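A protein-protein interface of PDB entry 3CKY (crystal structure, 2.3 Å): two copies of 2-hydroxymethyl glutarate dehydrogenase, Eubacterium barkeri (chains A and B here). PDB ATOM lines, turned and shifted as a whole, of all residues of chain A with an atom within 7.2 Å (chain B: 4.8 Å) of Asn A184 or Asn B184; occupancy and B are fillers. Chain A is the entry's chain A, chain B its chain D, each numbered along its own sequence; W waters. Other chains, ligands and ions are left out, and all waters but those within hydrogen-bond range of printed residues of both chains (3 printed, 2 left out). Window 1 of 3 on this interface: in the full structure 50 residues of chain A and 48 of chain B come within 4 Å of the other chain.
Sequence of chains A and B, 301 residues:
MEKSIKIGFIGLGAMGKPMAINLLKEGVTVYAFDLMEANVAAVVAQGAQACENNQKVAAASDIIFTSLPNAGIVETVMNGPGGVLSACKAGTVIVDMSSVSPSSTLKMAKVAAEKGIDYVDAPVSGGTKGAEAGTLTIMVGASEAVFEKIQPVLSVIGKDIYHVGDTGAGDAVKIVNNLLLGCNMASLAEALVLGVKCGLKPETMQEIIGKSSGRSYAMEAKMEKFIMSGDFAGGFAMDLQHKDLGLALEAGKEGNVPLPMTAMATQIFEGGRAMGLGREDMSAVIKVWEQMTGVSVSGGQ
Leu A180 touches Ser B187, and with the chains exchanged Ser A187 touches Leu B180.
Leu A181 touches Gly B214, and with the chains exchanged Gly A214 touches Leu B181.
Asn A184 touches Gly B214, and with the chains exchanged Gly A214 touches Asn B184.
Ser A216 touches its own counterpart, Ser B216.
Water W2 bridges the backbone carbonyl oxygen of Asn B184 (2.6 Å) and the side-chain amide oxygen of Asn A184 (2.8 Å).
Water W1 lies within hydrogen-bond range of O of Ser A213 (2.6 Å), O of Arg A215 (2.8 Å), ND2 of Asn B184 (2.9 Å) and N of Ala B218 (3.0 Å).
Water W3 bridges the backbone carbonyl oxygen of Asn A184 and the side-chain amide oxygen of Asn B184.
Of the printed residues of chain B, Leu A180 touches Ser B187 (3.7 Å), Leu B188 (3.7 Å) and Gly B214 (3.6 Å).
Of chain B, only Asn B184 (3.3 Å), Gly B214 (3.4 Å) and Arg B215 (3.9 Å) come within 4 Å of Asn A184.
Printed residues of chain B within 4 Å of Ser A216: Arg B215 (3.7 Å) and Ser B216 (3.9 Å).
Asn B184 touches just these residues of chain A: Asn A184 (3.3 Å), Gly A214 (3.3 Å) and Arg A215 (3.9 Å).
Ala B186 touches none of the printed residues of chain A.
Of the printed residues of chain A, Ser B187 touches Leu A180 (3.7 Å), Cys A183 (3.5 Å) and Met A261 (3.6 Å).
The nearest residue of chain B that does not touch Asn A184 is Ser B216 (4.2 Å).
The nearest residue of chain A that does not touch Asn B184 is Ser A216 (4.2 Å).
Leu A180 touches Ser B187 (CD2 to O, 3.7 Å).
Leu A180 touches Gly B214.
OG of Ser A187 touches CB of Cys B183 (3.3 Å).
O of Gly A214 touches CB of Leu B180 (3.6 Å).
Leu B181 touches Gly A214 (N to CA, 3.9 Å).
Asn B184 touches Arg A215 (ND2 to O, 3.9 Å).
Ser B216 touches Arg A215.
CB of Ser A216 touches CB of Ser B216 (3.9 Å).
O of Cys B183 touches CE of Met A261 (3.8 Å).
Met A261 touches Ser B187.
ND2 of Asn A177 lies within hydrogen-bond range of OD1 of Asn A178 (3.1 Å).
O of Leu A180 lies close to ND2 of Asn A184, at 3.2 Å.
OG of Ser A187 sits at hydrogen-bond distance from O of Cys A183 (3.0 Å).
The side-chain hydroxyl (OG) of Ser A216 lies within hydrogen-bond range of the backbone NH (N) of Met A219 (3.3 Å).
O of Leu B180 lies close to ND2 of Asn B184, 3.1 Å away.
O of Cys B183 lies within hydrogen-bond range of OG of Ser B187 (2.8 Å).
The side-chain amide oxygen (OD1) of Asn A177 lies within hydrogen-bond range of the backbone NH (N) of Gly B214 (2.7 Å).
The side-chain amide oxygen of Asn B184 sits close to the side-chain amide oxygen of Asn A184, at 3.3 Å.
The side-chain amide nitrogen (ND2) of Asn A184 sits at hydrogen-bond distance from the backbone carbonyl oxygen (O) of Gly B214.
The side-chain amide nitrogen (ND2) of Asn B184 lies within hydrogen-bond range of the backbone carbonyl oxygen (O) of Gly A214 (3.3 Å).
The backbone NH (N) of Tyr A217 lies within hydrogen-bond range of the backbone carbonyl oxygen (O) of Arg B215 (3.1 Å).
Hydrophobic or aromatic side chains of chain B that line the printed part of chain A: Leu B180 and Leu B181.
Among the printed residues, no Asp or Glu carboxylate lies within 4 Å of a Lys or Arg side-chain nitrogen of the other chain.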
ATOM      1  N   ASN A 177     -22.287  -4.505   8.880  1.00  0.00           N
ATOM      2  CA  ASN A 177     -21.808  -4.652   7.518  1.00  0.00           C
ATOM      3  C   ASN A 177     -20.428  -5.296   7.451  1.00  0.00           C
ATOM      4  O   ASN A 177     -20.217  -6.231   6.689  1.00  0.00           O
ATOM      5  CB  ASN A 177     -21.776  -3.306   6.790  1.00  0.00           C
ATOM      6  CG  ASN A 177     -21.216  -3.431   5.370  1.00  0.00           C
ATOM      7  OD1 ASN A 177     -21.893  -3.914   4.471  1.00  0.00           O
ATOM      8  ND2 ASN A 177     -19.958  -3.011   5.178  1.00  0.00           N
ATOM      9  N   ASN A 178     -19.492  -4.776   8.245  1.00  0.00           N
ATOM     10  CA  ASN A 178     -18.088  -5.224   8.222  1.00  0.00           C
ATOM     11  C   ASN A 178     -17.854  -6.617   8.787  1.00  0.00           C
ATOM     12  O   ASN A 178     -16.915  -7.293   8.394  1.00  0.00           O
ATOM     13  CB  ASN A 178     -17.226  -4.236   8.996  1.00  0.00           C
ATOM     14  CG  ASN A 178     -17.161  -2.880   8.328  1.00  0.00           C
ATOM     15  OD1 ASN A 178     -17.679  -2.686   7.229  1.00  0.00           O
ATOM     16  ND2 ASN A 178     -16.551  -1.926   9.000  1.00  0.00           N
ATOM     17  N   LEU A 179     -18.699  -7.003   9.735  1.00  0.00           N
ATOM     18  CA  LEU A 179     -18.819  -8.378  10.244  1.00  0.00           C
ATOM     19  C   LEU A 179     -19.138  -9.336   9.100  1.00  0.00           C
ATOM     20  O   LEU A 179     -18.532 -10.381   8.978  1.00  0.00           O
ATOM     21  CB  LEU A 179     -19.939  -8.386  11.294  1.00  0.00           C
ATOM     22  CG  LEU A 179     -20.641  -9.580  11.920  1.00  0.00           C
ATOM     23  CD1 LEU A 179     -21.651  -9.020  12.956  1.00  0.00           C
ATOM     24  CD2 LEU A 179     -21.331 -10.516  10.911  1.00  0.00           C
ATOM     25  N   LEU A 180     -20.101  -8.966   8.267  1.00  0.00           N
ATOM     26  CA  LEU A 180     -20.521  -9.814   7.163  1.00  0.00           C
ATOM     27  C   LEU A 180     -19.432  -9.923   6.112  1.00  0.00           C
ATOM     28  O   LEU A 180     -19.185 -11.023   5.611  1.00  0.00           O
ATOM     29  CB  LEU A 180     -21.825  -9.295   6.544  1.00  0.00           C
ATOM     30  CG  LEU A 180     -23.063  -9.475   7.429  1.00  0.00           C
ATOM     31  CD1 LEU A 180     -24.251  -8.689   6.869  1.00  0.00           C
ATOM     32  CD2 LEU A 180     -23.387 -10.973   7.572  1.00  0.00           C
ATOM     33  N   LEU A 181     -18.785  -8.794   5.786  1.00  0.00           N
ATOM     34  CA  LEU A 181     -17.613  -8.804   4.907  1.00  0.00           C
ATOM     35  C   LEU A 181     -16.546  -9.791   5.396  1.00  0.00           C
ATOM     36  O   LEU A 181     -16.042 -10.606   4.623  1.00  0.00           O
ATOM     37  CB  LEU A 181     -16.990  -7.405   4.805  1.00  0.00           C
ATOM     38  CG  LEU A 181     -15.715  -7.249   3.953  1.00  0.00           C
ATOM     39  CD1 LEU A 181     -15.942  -7.760   2.492  1.00  0.00           C
ATOM     40  CD2 LEU A 181     -15.229  -5.802   3.953  1.00  0.00           C
ATOM     41  N   GLY A 182     -16.196  -9.694   6.677  1.00  0.00           N
ATOM     42  CA  GLY A 182     -15.207 -10.574   7.283  1.00  0.00           C
ATOM     43  C   GLY A 182     -15.587 -12.038   7.274  1.00  0.00           C
ATOM     44  O   GLY A 182     -14.779 -12.885   6.903  1.00  0.00           O
ATOM     45  N   CYS A 183     -16.817 -12.334   7.671  1.00  0.00           N
ATOM     46  CA  CYS A 183     -17.319 -13.703   7.641  1.00  0.00           C
ATOM     47  C   CYS A 183     -17.324 -14.278   6.221  1.00  0.00           C
ATOM     48  O   CYS A 183     -16.911 -15.422   6.003  1.00  0.00           O
ATOM     49  CB  CYS A 183     -18.733 -13.780   8.220  1.00  0.00           C
ATOM     50  SG  CYS A 183     -18.861 -13.564  10.018  1.00  0.00           S
ATOM     51  N   ASN A 184     -17.802 -13.484   5.270  1.00  0.00           N
ATOM     52  CA  ASN A 184     -17.951 -13.936   3.895  1.00  0.00           C
ATOM     53  C   ASN A 184     -16.587 -14.256   3.311  1.00  0.00           C
ATOM     54  O   ASN A 184     -16.434 -15.228   2.582  1.00  0.00           O
ATOM     55  CB  ASN A 184     -18.685 -12.881   3.047  1.00  0.00           C
ATOM     56  CG  ASN A 184     -20.128 -12.696   3.456  1.00  0.00           C
ATOM     57  OD1 ASN A 184     -20.685 -13.486   4.222  1.00  0.00           O
ATOM     58  ND2 ASN A 184     -20.750 -11.648   2.942  1.00  0.00           N
ATOM     59  N   MET A 185     -15.586 -13.450   3.667  1.00  0.00           N
ATOM     60  CA  MET A 185     -14.230 -13.676   3.210  1.00  0.00           C
ATOM     61  C   MET A 185     -13.620 -14.927   3.840  1.00  0.00           C
ATOM     62  O   MET A 185     -13.034 -15.760   3.145  1.00  0.00           O
ATOM     63  CB  MET A 185     -13.357 -12.467   3.511  1.00  0.00           C
ATOM     64  CG  MET A 185     -11.866 -12.623   3.086  1.00  0.00           C
ATOM     65  SD  MET A 185     -11.578 -12.723   1.305  1.00  0.00           S
ATOM     66  CE  MET A 185     -10.998 -14.410   1.094  1.00  0.00           C
ATOM     67  N   ALA A 186     -13.759 -15.062   5.152  1.00  0.00           N
ATOM     68  CA  ALA A 186     -13.291 -16.261   5.837  1.00  0.00           C
ATOM     69  C   ALA A 186     -13.892 -17.544   5.215  1.00  0.00           C
ATOM     70  O   ALA A 186     -13.196 -18.535   5.021  1.00  0.00           O
ATOM     71  CB  ALA A 186     -13.609 -16.176   7.355  1.00  0.00           C
ATOM     72  N   SER A 187     -15.188 -17.514   4.917  1.00  0.00           N
ATOM     73  CA  SER A 187     -15.852 -18.651   4.286  1.00  0.00           C
ATOM     74  C   SER A 187     -15.295 -18.909   2.882  1.00  0.00           C
ATOM     75  O   SER A 187     -15.035 -20.044   2.493  1.00  0.00           O
ATOM     76  CB  SER A 187     -17.360 -18.405   4.209  1.00  0.00           C
ATOM     77  OG  SER A 187     -17.934 -18.202   5.491  1.00  0.00           O
ATOM     78  N   LEU A 188     -15.102 -17.834   2.133  1.00  0.00           N
ATOM     79  CA  LEU A 188     -14.542 -17.911   0.781  1.00  0.00           C
ATOM     80  C   LEU A 188     -13.148 -18.554   0.779  1.00  0.00           C
ATOM     81  O   LEU A 188     -12.831 -19.408  -0.069  1.00  0.00           O
ATOM     82  CB  LEU A 188     -14.489 -16.509   0.156  1.00  0.00           C
ATOM     83  CG  LEU A 188     -14.069 -16.441  -1.322  1.00  0.00           C
ATOM     84  CD1 LEU A 188     -15.032 -17.248  -2.228  1.00  0.00           C
ATOM     85  CD2 LEU A 188     -13.936 -14.996  -1.777  1.00  0.00           C
ATOM     86  N   ALA A 189     -12.333 -18.164   1.749  1.00  0.00           N
ATOM     87  CA  ALA A 189     -10.961 -18.660   1.854  1.00  0.00           C
ATOM     88  C   ALA A 189     -10.880 -20.198   1.845  1.00  0.00           C
ATOM     89  O   ALA A 189     -10.177 -20.794   0.997  1.00  0.00           O
ATOM     90  CB  ALA A 189     -10.301 -18.100   3.105  1.00  0.00           C
ATOM     91  N   SER A 213     -25.553 -18.785  -6.363  1.00  0.00           N
ATOM     92  CA  SER A 213     -26.077 -18.387  -5.066  1.00  0.00           C
ATOM     93  C   SER A 213     -25.007 -18.216  -3.993  1.00  0.00           C
ATOM     94  O   SER A 213     -25.273 -17.614  -2.958  1.00  0.00           O
ATOM     95  CB  SER A 213     -27.128 -19.404  -4.595  1.00  0.00           C
ATOM     96  OG  SER A 213     -26.586 -20.714  -4.606  1.00  0.00           O
ATOM     97  N   GLY A 214     -23.804 -18.729  -4.246  1.00  0.00           N
ATOM     98  CA  GLY A 214     -22.689 -18.595  -3.316  1.00  0.00           C
ATOM     99  C   GLY A 214     -22.010 -17.240  -3.354  1.00  0.00           C
ATOM    100  O   GLY A 214     -21.180 -16.957  -2.496  1.00  0.00           O
ATOM    101  N   ARG A 215     -22.350 -16.401  -4.337  1.00  0.00           N
ATOM    102  CA  ARG A 215     -21.639 -15.143  -4.550  1.00  0.00           C
ATOM    103  C   ARG A 215     -21.837 -14.138  -3.423  1.00  0.00           C
ATOM    104  O   ARG A 215     -22.824 -14.171  -2.699  1.00  0.00           O
ATOM    105  CB  ARG A 215     -21.995 -14.504  -5.887  1.00  0.00           C
ATOM    106  CG  ARG A 215     -23.395 -13.870  -5.970  1.00  0.00           C
ATOM    107  CD  ARG A 215     -23.593 -13.232  -7.338  1.00  0.00           C
ATOM    108  NE  ARG A 215     -24.985 -12.866  -7.588  1.00  0.00           N
ATOM    109  CZ  ARG A 215     -25.903 -13.669  -8.128  1.00  0.00           C
ATOM    110  NH1 ARG A 215     -25.599 -14.904  -8.519  1.00  0.00           N
ATOM    111  NH2 ARG A 215     -27.146 -13.221  -8.292  1.00  0.00           N
ATOM    112  N   SER A 216     -20.840 -13.282  -3.268  1.00  0.00           N
ATOM    113  CA  SER A 216     -20.868 -12.207  -2.300  1.00  0.00           C
ATOM    114  C   SER A 216     -20.010 -11.076  -2.829  1.00  0.00           C
ATOM    115  O   SER A 216     -19.216 -11.273  -3.742  1.00  0.00           O
ATOM    116  CB  SER A 216     -20.335 -12.686  -0.946  1.00  0.00           C
ATOM    117  OG  SER A 216     -18.966 -13.086  -1.018  1.00  0.00           O
ATOM    118  N   TYR A 217     -20.175  -9.887  -2.269  1.00  0.00           N
ATOM    119  CA  TYR A 217     -19.293  -8.787  -2.601  1.00  0.00           C
ATOM    120  C   TYR A 217     -17.833  -9.125  -2.250  1.00  0.00           C
ATOM    121  O   TYR A 217     -16.929  -8.823  -3.009  1.00  0.00           O
ATOM    122  CB  TYR A 217     -19.737  -7.497  -1.908  1.00  0.00           C
ATOM    123  CG  TYR A 217     -18.766  -6.394  -2.144  1.00  0.00           C
ATOM    124  CD1 TYR A 217     -18.804  -5.653  -3.314  1.00  0.00           C
ATOM    125  CD2 TYR A 217     -17.764  -6.126  -1.232  1.00  0.00           C
ATOM    126  CE1 TYR A 217     -17.875  -4.642  -3.557  1.00  0.00           C
ATOM    127  CE2 TYR A 217     -16.842  -5.125  -1.461  1.00  0.00           C
ATOM    128  CZ  TYR A 217     -16.912  -4.391  -2.619  1.00  0.00           C
ATOM    129  OH  TYR A 217     -15.997  -3.412  -2.838  1.00  0.00           O
ATOM    130  N   ALA A 218     -17.620  -9.758  -1.100  1.00  0.00           N
ATOM    131  CA  ALA A 218     -16.283 -10.267  -0.719  1.00  0.00           C
ATOM    132  C   ALA A 218     -15.592 -10.992  -1.879  1.00  0.00           C
ATOM    133  O   ALA A 218     -14.457 -10.677  -2.241  1.00  0.00           O
ATOM    134  CB  ALA A 218     -16.369 -11.171   0.483  1.00  0.00           C
ATOM    135  N   MET A 219     -16.281 -11.952  -2.479  1.00  0.00           N
ATOM    136  CA  MET A 219     -15.724 -12.662  -3.609  1.00  0.00           C
ATOM    137  C   MET A 219     -15.502 -11.733  -4.812  1.00  0.00           C
ATOM    138  O   MET A 219     -14.453 -11.798  -5.465  1.00  0.00           O
ATOM    139  CB  MET A 219     -16.616 -13.832  -3.998  1.00  0.00           C
ATOM    140  CG  MET A 219     -16.102 -14.592  -5.198  1.00  0.00           C
ATOM    141  SD  MET A 219     -17.017 -16.085  -5.499  1.00  0.00           S
ATOM    142  CE  MET A 219     -15.999 -16.845  -6.758  1.00  0.00           C
ATOM    143  N   MET A 261     -20.288 -17.501  14.076  1.00  0.00           N
ATOM    144  CA  MET A 261     -19.600 -17.352  12.787  1.00  0.00           C
ATOM    145  C   MET A 261     -18.581 -16.230  12.841  1.00  0.00           C
ATOM    146  O   MET A 261     -17.475 -16.358  12.317  1.00  0.00           O
ATOM    147  CB  MET A 261     -20.600 -17.064  11.663  1.00  0.00           C
ATOM    148  CG  MET A 261     -21.605 -18.175  11.432  1.00  0.00           C
ATOM    149  SD  MET A 261     -20.887 -19.716  10.870  1.00  0.00           S
ATOM    150  CE  MET A 261     -20.443 -19.294   9.163  1.00  0.00           C
ATOM    151  N   ALA A 265     -14.568 -16.550  12.409  1.00  0.00           N
ATOM    152  CA  ALA A 265     -13.877 -15.683  11.433  1.00  0.00           C
ATOM    153  C   ALA A 265     -12.749 -14.909  12.104  1.00  0.00           C
ATOM    154  O   ALA A 265     -11.667 -14.784  11.558  1.00  0.00           O
ATOM    155  CB  ALA A 265     -14.866 -14.710  10.749  1.00  0.00           C
ATOM    156  N   PHE A 269      -8.757 -15.047  10.976  1.00  0.00           N
ATOM    157  CA  PHE A 269      -7.972 -13.854  10.677  1.00  0.00           C
ATOM    158  C   PHE A 269      -6.821 -13.633  11.669  1.00  0.00           C
ATOM    159  O   PHE A 269      -5.797 -13.073  11.291  1.00  0.00           O
ATOM    160  CB  PHE A 269      -8.842 -12.599  10.629  1.00  0.00           C
ATOM    161  CG  PHE A 269      -9.612 -12.450   9.359  1.00  0.00           C
ATOM    162  CD1 PHE A 269      -8.963 -12.141   8.169  1.00  0.00           C
ATOM    163  CD2 PHE A 269     -10.991 -12.607   9.347  1.00  0.00           C
ATOM    164  CE1 PHE A 269      -9.675 -11.970   6.982  1.00  0.00           C
ATOM    165  CE2 PHE A 269     -11.712 -12.452   8.179  1.00  0.00           C
ATOM    166  CZ  PHE A 269     -11.044 -12.129   6.979  1.00  0.00           C
ATOM    167  N   LEU B 180     -20.910 -21.966   0.368  1.00  0.00           N
ATOM    168  CA  LEU B 180     -20.834 -20.523   0.535  1.00  0.00           C
ATOM    169  C   LEU B 180     -22.222 -19.944   0.800  1.00  0.00           C
ATOM    170  O   LEU B 180     -22.364 -19.056   1.633  1.00  0.00           O
ATOM    171  CB  LEU B 180     -20.187 -19.859  -0.685  1.00  0.00           C
ATOM    172  CG  LEU B 180     -18.678 -20.128  -0.843  1.00  0.00           C
ATOM    173  CD1 LEU B 180     -18.163 -19.632  -2.232  1.00  0.00           C
ATOM    174  CD2 LEU B 180     -17.899 -19.505   0.313  1.00  0.00           C
ATOM    175  N   LEU B 181     -23.237 -20.445   0.093  1.00  0.00           N
ATOM    176  CA  LEU B 181     -24.614 -20.029   0.351  1.00  0.00           C
ATOM    177  C   LEU B 181     -24.989 -20.247   1.829  1.00  0.00           C
ATOM    178  O   LEU B 181     -25.513 -19.347   2.488  1.00  0.00           O
ATOM    179  CB  LEU B 181     -25.582 -20.799  -0.550  1.00  0.00           C
ATOM    180  CG  LEU B 181     -27.078 -20.560  -0.312  1.00  0.00           C
ATOM    181  CD1 LEU B 181     -27.416 -19.079  -0.442  1.00  0.00           C
ATOM    182  CD2 LEU B 181     -27.955 -21.422  -1.236  1.00  0.00           C
ATOM    183  N   GLY B 182     -24.705 -21.456   2.325  1.00  0.00           N
ATOM    184  CA  GLY B 182     -24.980 -21.819   3.712  1.00  0.00           C
ATOM    185  C   GLY B 182     -24.230 -20.989   4.731  1.00  0.00           C
ATOM    186  O   GLY B 182     -24.804 -20.559   5.717  1.00  0.00           O
ATOM    187  N   CYS B 183     -22.934 -20.792   4.502  1.00  0.00           N
ATOM    188  CA  CYS B 183     -22.103 -19.962   5.400  1.00  0.00           C
ATOM    189  C   CYS B 183     -22.539 -18.513   5.396  1.00  0.00           C
ATOM    190  O   CYS B 183     -22.585 -17.850   6.442  1.00  0.00           O
ATOM    191  CB  CYS B 183     -20.631 -20.018   5.005  1.00  0.00           C
ATOM    192  SG  CYS B 183     -19.860 -21.573   5.374  1.00  0.00           S
ATOM    193  N   ASN B 184     -22.848 -18.004   4.215  1.00  0.00           N
ATOM    194  CA  ASN B 184     -23.286 -16.619   4.096  1.00  0.00           C
ATOM    195  C   ASN B 184     -24.605 -16.387   4.830  1.00  0.00           C
ATOM    196  O   ASN B 184     -24.796 -15.345   5.464  1.00  0.00           O
ATOM    197  CB  ASN B 184     -23.394 -16.192   2.631  1.00  0.00           C
ATOM    198  CG  ASN B 184     -22.049 -16.195   1.916  1.00  0.00           C
ATOM    199  OD1 ASN B 184     -20.983 -16.265   2.559  1.00  0.00           O
ATOM    200  ND2 ASN B 184     -22.090 -16.151   0.572  1.00  0.00           N
ATOM    201  N   MET B 185     -25.493 -17.369   4.767  1.00  0.00           N
ATOM    202  CA  MET B 185     -26.775 -17.283   5.460  1.00  0.00           C
ATOM    203  C   MET B 185     -26.601 -17.377   6.978  1.00  0.00           C
ATOM    204  O   MET B 185     -27.246 -16.635   7.721  1.00  0.00           O
ATOM    205  CB  MET B 185     -27.717 -18.384   4.987  1.00  0.00           C
ATOM    206  CG  MET B 185     -29.093 -18.388   5.698  1.00  0.00           C
ATOM    207  SD  MET B 185     -30.092 -16.903   5.386  1.00  0.00           S
ATOM    208  CE  MET B 185     -30.204 -16.143   7.018  1.00  0.00           C
ATOM    209  N   ALA B 186     -25.775 -18.318   7.431  1.00  0.00           N
ATOM    210  CA  ALA B 186     -25.537 -18.489   8.844  1.00  0.00           C
ATOM    211  C   ALA B 186     -24.966 -17.198   9.446  1.00  0.00           C
ATOM    212  O   ALA B 186     -25.326 -16.798  10.550  1.00  0.00           O
ATOM    213  CB  ALA B 186     -24.600 -19.672   9.078  1.00  0.00           C
ATOM    214  N   SER B 187     -24.068 -16.557   8.710  1.00  0.00           N
ATOM    215  CA  SER B 187     -23.438 -15.315   9.149  1.00  0.00           C
ATOM    216  C   SER B 187     -24.466 -14.195   9.169  1.00  0.00           C
ATOM    217  O   SER B 187     -24.532 -13.403  10.119  1.00  0.00           O
ATOM    218  CB  SER B 187     -22.302 -14.958   8.206  1.00  0.00           C
ATOM    219  OG  SER B 187     -21.382 -16.031   8.120  1.00  0.00           O
ATOM    220  N   LEU B 188     -25.278 -14.147   8.116  1.00  0.00           N
ATOM    221  CA  LEU B 188     -26.376 -13.176   8.041  1.00  0.00           C
ATOM    222  C   LEU B 188     -27.329 -13.281   9.222  1.00  0.00           C
ATOM    223  O   LEU B 188     -27.757 -12.254   9.749  1.00  0.00           O
ATOM    224  CB  LEU B 188     -27.160 -13.352   6.733  1.00  0.00           C
ATOM    225  CG  LEU B 188     -28.260 -12.320   6.445  1.00  0.00           C
ATOM    226  CD1 LEU B 188     -27.653 -10.909   6.371  1.00  0.00           C
ATOM    227  CD2 LEU B 188     -29.043 -12.677   5.140  1.00  0.00           C
ATOM    228  N   GLY B 214     -20.898  -5.855   2.834  1.00  0.00           N
ATOM    229  CA  GLY B 214     -21.419  -7.023   3.531  1.00  0.00           C
ATOM    230  C   GLY B 214     -22.409  -7.851   2.721  1.00  0.00           C
ATOM    231  O   GLY B 214     -22.800  -8.951   3.135  1.00  0.00           O
ATOM    232  N   ARG B 215     -22.805  -7.329   1.561  1.00  0.00           N
ATOM    233  CA  ARG B 215     -23.856  -7.931   0.746  1.00  0.00           C
ATOM    234  C   ARG B 215     -23.470  -9.307   0.189  1.00  0.00           C
ATOM    235  O   ARG B 215     -22.303  -9.593  -0.050  1.00  0.00           O
ATOM    236  CB  ARG B 215     -24.259  -6.983  -0.402  1.00  0.00           C
ATOM    237  CG  ARG B 215     -23.476  -7.190  -1.681  1.00  0.00           C
ATOM    238  CD  ARG B 215     -23.908  -6.246  -2.751  1.00  0.00           C
ATOM    239  NE  ARG B 215     -23.252  -4.970  -2.523  1.00  0.00           N
ATOM    240  CZ  ARG B 215     -22.358  -4.413  -3.323  1.00  0.00           C
ATOM    241  NH1 ARG B 215     -22.021  -4.983  -4.477  1.00  0.00           N
ATOM    242  NH2 ARG B 215     -21.820  -3.258  -2.962  1.00  0.00           N
ATOM    243  N   SER B 216     -24.482 -10.156   0.020  1.00  0.00           N
ATOM    244  CA  SER B 216     -24.322 -11.469  -0.590  1.00  0.00           C
ATOM    245  C   SER B 216     -25.616 -11.839  -1.274  1.00  0.00           C
ATOM    246  O   SER B 216     -26.646 -11.240  -0.995  1.00  0.00           O
ATOM    247  CB  SER B 216     -23.966 -12.508   0.464  1.00  0.00           C
ATOM    248  OG  SER B 216     -24.973 -12.631   1.432  1.00  0.00           O
ATOM    249  N   ALA B 218     -27.165 -14.588  -0.705  1.00  0.00           N
ATOM    250  CA  ALA B 218     -27.923 -15.079   0.447  1.00  0.00           C
ATOM    251  C   ALA B 218     -28.843 -13.997   1.019  1.00  0.00           C
ATOM    252  O   ALA B 218     -30.048 -14.219   1.195  1.00  0.00           O
ATOM    253  CB  ALA B 218     -26.967 -15.599   1.522  1.00  0.00           C
HETATM  254  O   HOH W   1     -24.473 -15.874  -1.140  1.00  0.00           O
HETATM  255  O   HOH W   2     -23.368 -13.225   4.889  1.00  0.00           O
HETATM  256  O   HOH W   3     -18.602 -16.038   1.224  1.00  0.00           O
